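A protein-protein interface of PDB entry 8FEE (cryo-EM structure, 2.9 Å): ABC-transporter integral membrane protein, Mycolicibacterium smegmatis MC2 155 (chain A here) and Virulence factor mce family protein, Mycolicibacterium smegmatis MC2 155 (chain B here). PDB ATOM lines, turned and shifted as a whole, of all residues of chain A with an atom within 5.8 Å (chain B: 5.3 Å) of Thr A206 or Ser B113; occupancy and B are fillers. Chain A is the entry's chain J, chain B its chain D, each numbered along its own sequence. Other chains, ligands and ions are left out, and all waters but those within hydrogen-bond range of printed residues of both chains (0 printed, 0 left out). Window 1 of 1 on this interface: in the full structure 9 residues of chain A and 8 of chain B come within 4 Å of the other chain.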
ATOM      1  N   ALA A 107      11.608  -5.516 -13.290  1.00  0.00           N
ATOM      2  CA  ALA A 107      11.784  -6.499 -14.350  1.00  0.00           C
ATOM      3  C   ALA A 107      10.532  -7.332 -14.582  1.00  0.00           C
ATOM      4  O   ALA A 107      10.428  -7.996 -15.619  1.00  0.00           O
ATOM      5  CB  ALA A 107      12.962  -7.418 -14.031  1.00  0.00           C
ATOM      6  N   GLN A 202      14.268  -0.425 -21.208  1.00  0.00           N
ATOM      7  CA  GLN A 202      14.500  -1.734 -20.618  1.00  0.00           C
ATOM      8  C   GLN A 202      15.039  -2.690 -21.678  1.00  0.00           C
ATOM      9  O   GLN A 202      14.821  -2.506 -22.877  1.00  0.00           O
ATOM     10  CB  GLN A 202      13.210  -2.288 -20.009  1.00  0.00           C
ATOM     11  CG  GLN A 202      13.424  -3.444 -19.040  1.00  0.00           C
ATOM     12  CD  GLN A 202      12.131  -4.107 -18.616  1.00  0.00           C
ATOM     13  OE1 GLN A 202      11.455  -4.743 -19.423  1.00  0.00           O
ATOM     14  NE2 GLN A 202      11.782  -3.965 -17.344  1.00  0.00           N
ATOM     15  N   SER A 203      15.768  -3.707 -21.226  1.00  0.00           N
ATOM     16  CA  SER A 203      16.306  -4.700 -22.143  1.00  0.00           C
ATOM     17  C   SER A 203      15.182  -5.513 -22.770  1.00  0.00           C
ATOM     18  O   SER A 203      14.198  -5.854 -22.108  1.00  0.00           O
ATOM     19  CB  SER A 203      17.280  -5.624 -21.417  1.00  0.00           C
ATOM     20  OG  SER A 203      16.666  -6.224 -20.292  1.00  0.00           O
ATOM     21  N   VAL A 204      15.328  -5.815 -24.061  1.00  0.00           N
ATOM     22  CA  VAL A 204      14.327  -6.626 -24.744  1.00  0.00           C
ATOM     23  C   VAL A 204      14.376  -8.071 -24.260  1.00  0.00           C
ATOM     24  O   VAL A 204      13.346  -8.757 -24.233  1.00  0.00           O
ATOM     25  CB  VAL A 204      14.504  -6.515 -26.273  1.00  0.00           C
ATOM     26  CG1 VAL A 204      15.832  -7.108 -26.724  1.00  0.00           C
ATOM     27  CG2 VAL A 204      13.339  -7.170 -27.004  1.00  0.00           C
ATOM     28  N   GLY A 205      15.557  -8.555 -23.865  1.00  0.00           N
ATOM     29  CA  GLY A 205      15.681  -9.945 -23.450  1.00  0.00           C
ATOM     30  C   GLY A 205      14.887 -10.268 -22.201  1.00  0.00           C
ATOM     31  O   GLY A 205      14.179 -11.275 -22.144  1.00  0.00           O
ATOM     32  N   THR A 206      14.988  -9.411 -21.181  1.00  0.00           N
ATOM     33  CA  THR A 206      14.247  -9.636 -19.944  1.00  0.00           C
ATOM     34  C   THR A 206      12.744  -9.557 -20.178  1.00  0.00           C
ATOM     35  O   THR A 206      11.980 -10.387 -19.665  1.00  0.00           O
ATOM     36  CB  THR A 206      14.681  -8.622 -18.886  1.00  0.00           C
ATOM     37  OG1 THR A 206      16.076  -8.787 -18.612  1.00  0.00           O
ATOM     38  CG2 THR A 206      13.893  -8.810 -17.600  1.00  0.00           C
ATOM     39  N   TYR A 207      12.305  -8.569 -20.962  1.00  0.00           N
ATOM     40  CA  TYR A 207      10.885  -8.429 -21.262  1.00  0.00           C
ATOM     41  C   TYR A 207      10.360  -9.662 -21.985  1.00  0.00           C
ATOM     42  O   TYR A 207       9.323 -10.220 -21.610  1.00  0.00           O
ATOM     43  CB  TYR A 207      10.645  -7.173 -22.102  1.00  0.00           C
ATOM     44  CG  TYR A 207       9.182  -6.826 -22.286  1.00  0.00           C
ATOM     45  CD1 TYR A 207       8.431  -7.401 -23.303  1.00  0.00           C
ATOM     46  CD2 TYR A 207       8.556  -5.919 -21.447  1.00  0.00           C
ATOM     47  CE1 TYR A 207       7.100  -7.093 -23.468  1.00  0.00           C
ATOM     48  CE2 TYR A 207       7.224  -5.599 -21.611  1.00  0.00           C
ATOM     49  CZ  TYR A 207       6.501  -6.190 -22.619  1.00  0.00           C
ATOM     50  OH  TYR A 207       5.173  -5.874 -22.781  1.00  0.00           O
ATOM     51  N   GLU A 208      11.073 -10.103 -23.024  1.00  0.00           N
ATOM     52  CA  GLU A 208      10.628 -11.264 -23.784  1.00  0.00           C
ATOM     53  C   GLU A 208      10.639 -12.524 -22.931  1.00  0.00           C
ATOM     54  O   GLU A 208       9.724 -13.347 -23.029  1.00  0.00           O
ATOM     55  CB  GLU A 208      11.495 -11.448 -25.027  1.00  0.00           C
ATOM     56  CG  GLU A 208      11.218 -10.433 -26.121  1.00  0.00           C
ATOM     57  CD  GLU A 208      11.844 -10.819 -27.443  1.00  0.00           C
ATOM     58  OE1 GLU A 208      12.401 -11.932 -27.535  1.00  0.00           O
ATOM     59  OE2 GLU A 208      11.777 -10.010 -28.392  1.00  0.00           O
ATOM     60  N   HIS A 209      11.656 -12.688 -22.079  1.00  0.00           N
ATOM     61  CA  HIS A 209      11.708 -13.863 -21.216  1.00  0.00           C
ATOM     62  C   HIS A 209      10.512 -13.907 -20.277  1.00  0.00           C
ATOM     63  O   HIS A 209       9.806 -14.918 -20.205  1.00  0.00           O
ATOM     64  CB  HIS A 209      13.006 -13.884 -20.413  1.00  0.00           C
ATOM     65  CG  HIS A 209      12.985 -14.851 -19.270  1.00  0.00           C
ATOM     66  ND1 HIS A 209      13.293 -16.186 -19.419  1.00  0.00           N
ATOM     67  CD2 HIS A 209      12.681 -14.678 -17.961  1.00  0.00           C
ATOM     68  CE1 HIS A 209      13.185 -16.793 -18.251  1.00  0.00           C
ATOM     69  NE2 HIS A 209      12.816 -15.901 -17.349  1.00  0.00           N
ATOM     70  N   TYR A 210      10.272 -12.818 -19.542  1.00  0.00           N
ATOM     71  CA  TYR A 210       9.175 -12.827 -18.579  1.00  0.00           C
ATOM     72  C   TYR A 210       7.827 -12.953 -19.276  1.00  0.00           C
ATOM     73  O   TYR A 210       6.937 -13.666 -18.793  1.00  0.00           O
ATOM     74  CB  TYR A 210       9.228 -11.577 -17.704  1.00  0.00           C
ATOM     75  CG  TYR A 210      10.196 -11.708 -16.551  1.00  0.00           C
ATOM     76  CD1 TYR A 210      11.542 -11.418 -16.715  1.00  0.00           C
ATOM     77  CD2 TYR A 210       9.767 -12.144 -15.306  1.00  0.00           C
ATOM     78  CE1 TYR A 210      12.433 -11.545 -15.667  1.00  0.00           C
ATOM     79  CE2 TYR A 210      10.649 -12.276 -14.254  1.00  0.00           C
ATOM     80  CZ  TYR A 210      11.980 -11.974 -14.439  1.00  0.00           C
ATOM     81  OH  TYR A 210      12.863 -12.101 -13.393  1.00  0.00           O
ATOM     82  N   PHE A 211       7.664 -12.287 -20.425  1.00  0.00           N
ATOM     83  CA  PHE A 211       6.414 -12.369 -21.168  1.00  0.00           C
ATOM     84  C   PHE A 211       6.152 -13.794 -21.643  1.00  0.00           C
ATOM     85  O   PHE A 211       5.093 -14.365 -21.369  1.00  0.00           O
ATOM     86  CB  PHE A 211       6.455 -11.393 -22.345  1.00  0.00           C
ATOM     87  CG  PHE A 211       5.244 -11.445 -23.227  1.00  0.00           C
ATOM     88  CD1 PHE A 211       4.053 -10.873 -22.822  1.00  0.00           C
ATOM     89  CD2 PHE A 211       5.303 -12.046 -24.471  1.00  0.00           C
ATOM     90  CE1 PHE A 211       2.941 -10.914 -23.632  1.00  0.00           C
ATOM     91  CE2 PHE A 211       4.195 -12.091 -25.285  1.00  0.00           C
ATOM     92  CZ  PHE A 211       3.011 -11.524 -24.865  1.00  0.00           C
ATOM     93  N   TYR B  60      20.083 -12.976 -20.837  1.00  0.00           N
ATOM     94  CA  TYR B  60      19.421 -13.187 -22.113  1.00  0.00           C
ATOM     95  C   TYR B  60      20.039 -12.277 -23.160  1.00  0.00           C
ATOM     96  O   TYR B  60      20.637 -11.251 -22.824  1.00  0.00           O
ATOM     97  CB  TYR B  60      17.916 -12.905 -21.991  1.00  0.00           C
ATOM     98  CG  TYR B  60      17.302 -13.508 -20.750  1.00  0.00           C
ATOM     99  CD1 TYR B  60      17.247 -14.883 -20.578  1.00  0.00           C
ATOM    100  CD2 TYR B  60      16.791 -12.701 -19.745  1.00  0.00           C
ATOM    101  CE1 TYR B  60      16.695 -15.437 -19.442  1.00  0.00           C
ATOM    102  CE2 TYR B  60      16.235 -13.246 -18.607  1.00  0.00           C
ATOM    103  CZ  TYR B  60      16.190 -14.614 -18.460  1.00  0.00           C
ATOM    104  OH  TYR B  60      15.638 -15.160 -17.326  1.00  0.00           O
ATOM    105  N   ASP B  63      20.490  -8.075 -23.222  1.00  0.00           N
ATOM    106  CA  ASP B  63      20.756  -7.482 -21.922  1.00  0.00           C
ATOM    107  C   ASP B  63      21.937  -6.522 -22.007  1.00  0.00           C
ATOM    108  O   ASP B  63      22.788  -6.614 -22.897  1.00  0.00           O
ATOM    109  CB  ASP B  63      21.030  -8.566 -20.878  1.00  0.00           C
ATOM    110  CG  ASP B  63      19.782  -8.976 -20.122  1.00  0.00           C
ATOM    111  OD1 ASP B  63      18.746  -8.297 -20.269  1.00  0.00           O
ATOM    112  OD2 ASP B  63      19.836  -9.978 -19.380  1.00  0.00           O
ATOM    113  N   LEU B 106      26.543  -9.556 -13.329  1.00  0.00           N
ATOM    114  CA  LEU B 106      26.064  -8.974 -12.088  1.00  0.00           C
ATOM    115  C   LEU B 106      24.546  -9.043 -12.022  1.00  0.00           C
ATOM    116  O   LEU B 106      23.853  -8.911 -13.038  1.00  0.00           O
ATOM    117  CB  LEU B 106      26.507  -7.515 -11.945  1.00  0.00           C
ATOM    118  CG  LEU B 106      27.971  -7.176 -12.215  1.00  0.00           C
ATOM    119  CD1 LEU B 106      28.173  -5.678 -12.122  1.00  0.00           C
ATOM    120  CD2 LEU B 106      28.875  -7.900 -11.237  1.00  0.00           C
ATOM    121  N   ASN B 107      24.047  -9.230 -10.802  1.00  0.00           N
ATOM    122  CA  ASN B 107      22.630  -9.125 -10.479  1.00  0.00           C
ATOM    123  C   ASN B 107      22.450  -7.857  -9.657  1.00  0.00           C
ATOM    124  O   ASN B 107      22.745  -7.856  -8.452  1.00  0.00           O
ATOM    125  CB  ASN B 107      22.151 -10.352  -9.700  1.00  0.00           C
ATOM    126  CG  ASN B 107      20.647 -10.378  -9.518  1.00  0.00           C
ATOM    127  OD1 ASN B 107      19.916  -9.669 -10.207  1.00  0.00           O
ATOM    128  ND2 ASN B 107      20.178 -11.199  -8.587  1.00  0.00           N
ATOM    129  N   PRO B 108      22.003  -6.752 -10.263  1.00  0.00           N
ATOM    130  CA  PRO B 108      21.991  -5.466  -9.543  1.00  0.00           C
ATOM    131  C   PRO B 108      21.178  -5.455  -8.259  1.00  0.00           C
ATOM    132  O   PRO B 108      21.584  -4.801  -7.291  1.00  0.00           O
ATOM    133  CB  PRO B 108      21.406  -4.504 -10.585  1.00  0.00           C
ATOM    134  CG  PRO B 108      21.802  -5.098 -11.890  1.00  0.00           C
ATOM    135  CD  PRO B 108      21.710  -6.585 -11.696  1.00  0.00           C
ATOM    136  N   VAL B 111      15.313  -8.274  -7.814  1.00  0.00           N
ATOM    137  CA  VAL B 111      14.744  -8.543  -9.128  1.00  0.00           C
ATOM    138  C   VAL B 111      15.257  -7.474 -10.079  1.00  0.00           C
ATOM    139  O   VAL B 111      14.945  -6.288  -9.913  1.00  0.00           O
ATOM    140  CB  VAL B 111      13.209  -8.559  -9.102  1.00  0.00           C
ATOM    141  CG1 VAL B 111      12.671  -8.909 -10.475  1.00  0.00           C
ATOM    142  CG2 VAL B 111      12.702  -9.542  -8.062  1.00  0.00           C
ATOM    143  N   ALA B 112      16.032  -7.892 -11.072  1.00  0.00           N
ATOM    144  CA  ALA B 112      16.637  -6.971 -12.025  1.00  0.00           C
ATOM    145  C   ALA B 112      17.085  -7.772 -13.238  1.00  0.00           C
ATOM    146  O   ALA B 112      16.898  -8.989 -13.309  1.00  0.00           O
ATOM    147  CB  ALA B 112      17.804  -6.207 -11.398  1.00  0.00           C
ATOM    148  N   SER B 113      17.682  -7.075 -14.198  1.00  0.00           N
ATOM    149  CA  SER B 113      18.260  -7.704 -15.375  1.00  0.00           C
ATOM    150  C   SER B 113      19.766  -7.808 -15.178  1.00  0.00           C
ATOM    151  O   SER B 113      20.438  -6.794 -14.965  1.00  0.00           O
ATOM    152  CB  SER B 113      17.931  -6.910 -16.639  1.00  0.00           C
ATOM    153  OG  SER B 113      18.436  -5.590 -16.561  1.00  0.00           O
ATOM    154  N   ARG B 114      20.285  -9.030 -15.235  1.00  0.00           N
ATOM    155  CA  ARG B 114      21.709  -9.251 -15.038  1.00  0.00           C
ATOM    156  C   ARG B 114      22.496  -8.639 -16.188  1.00  0.00           C
ATOM    157  O   ARG B 114      22.076  -8.695 -17.347  1.00  0.00           O
ATOM    158  CB  ARG B 114      21.995 -10.745 -14.922  1.00  0.00           C
ATOM    159  CG  ARG B 114      21.118 -11.427 -13.896  1.00  0.00           C
ATOM    160  CD  ARG B 114      21.700 -12.746 -13.449  1.00  0.00           C
ATOM    161  NE  ARG B 114      20.982 -13.282 -12.301  1.00  0.00           N
ATOM    162  CZ  ARG B 114      21.360 -14.350 -11.616  1.00  0.00           C
ATOM    163  NH1 ARG B 114      22.445 -15.031 -11.944  1.00  0.00           N
ATOM    164  NH2 ARG B 114      20.632 -14.746 -10.576  1.00  0.00           N
ATOM    165  N   VAL B 115      23.640  -8.039 -15.865  1.00  0.00           N
ATOM    166  CA  VAL B 115      24.407  -7.286 -16.848  1.00  0.00           C
ATOM    167  C   VAL B 115      25.859  -7.734 -16.827  1.00  0.00           C
ATOM    168  O   VAL B 115      26.397  -8.118 -15.786  1.00  0.00           O
ATOM    169  CB  VAL B 115      24.309  -5.765 -16.598  1.00  0.00           C
ATOM    170  CG1 VAL B 115      22.887  -5.279 -16.815  1.00  0.00           C
ATOM    171  CG2 VAL B 115      24.763  -5.435 -15.189  1.00  0.00           C
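CB of Ala A107 touches CG1 of Val B111 (3.9 Å). Ser A203 touches Ser B113. O of Gly A205 touches CD2 of Tyr B60 (3.8 Å). Thr A206 touches Tyr B60. Thr A206 touches Ser B113.
Of the 11 printed residues of chain A, 5 touch a printed residue of chain B. Hydrophobic or aromatic side chains of chain A that line the printed part of chain B: Ala A107 and His A209. Printed residues of chain B that touch a printed residue of chain A: Tyr B60, Asp B63, Val B111 and Ser B113. Among the printed residues, 8 pairs touch across the chains. Among the printed residues, no Asp or Glu carboxylate lies within 4 Å of a Lys or Arg side-chain nitrogen of the other chain.
The backbone NH (N) of Tyr B60 lies within hydrogen-bond range of the side-chain carboxylate (OD2) of Asp B63 (3.3 Å). The side-chain hydroxyl (OG1) of Thr A206 lies within hydrogen-bond range of the side-chain hydroxyl (OG) of Ser A203, 3.1 Å away.
OD1 of Asp B63 is in hydrogen-bond range of OG1 of Thr A206, 3.2 Å away. A ring nitrogen (NE2) of His A209 lies within hydrogen-bond range of the side-chain hydroxyl of Tyr B60, at 2.9 Å. The side-chain carboxylate (OD1) of Asp B63 lies within hydrogen-bond range of the side-chain hydroxyl (OG) of Ser A203.
Of the printed residues of chain B, Thr A206 touches Tyr B60, Asp B63 and Ser B113. Of chain A, only Ser A203 (3.9 Å) and Thr A206 (3.3 Å) come within 4 Å of Ser B113. Of the printed residues of chain B, His A209 touches Tyr B60 (2.9 Å). Of the printed residues of chain A, Asp B63 touches Ser A203 and Thr A206. Of the printed residues of chain B, Ala A107 touches Val B111. Of the printed residues of chain B, Gly A205 touches Tyr B60 (3.8 Å). Arg B114 touches none of the printed residues of chain A. The nearest residue of chain A that does not touch Ser B113 is Ala A107 (4.7 Å).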
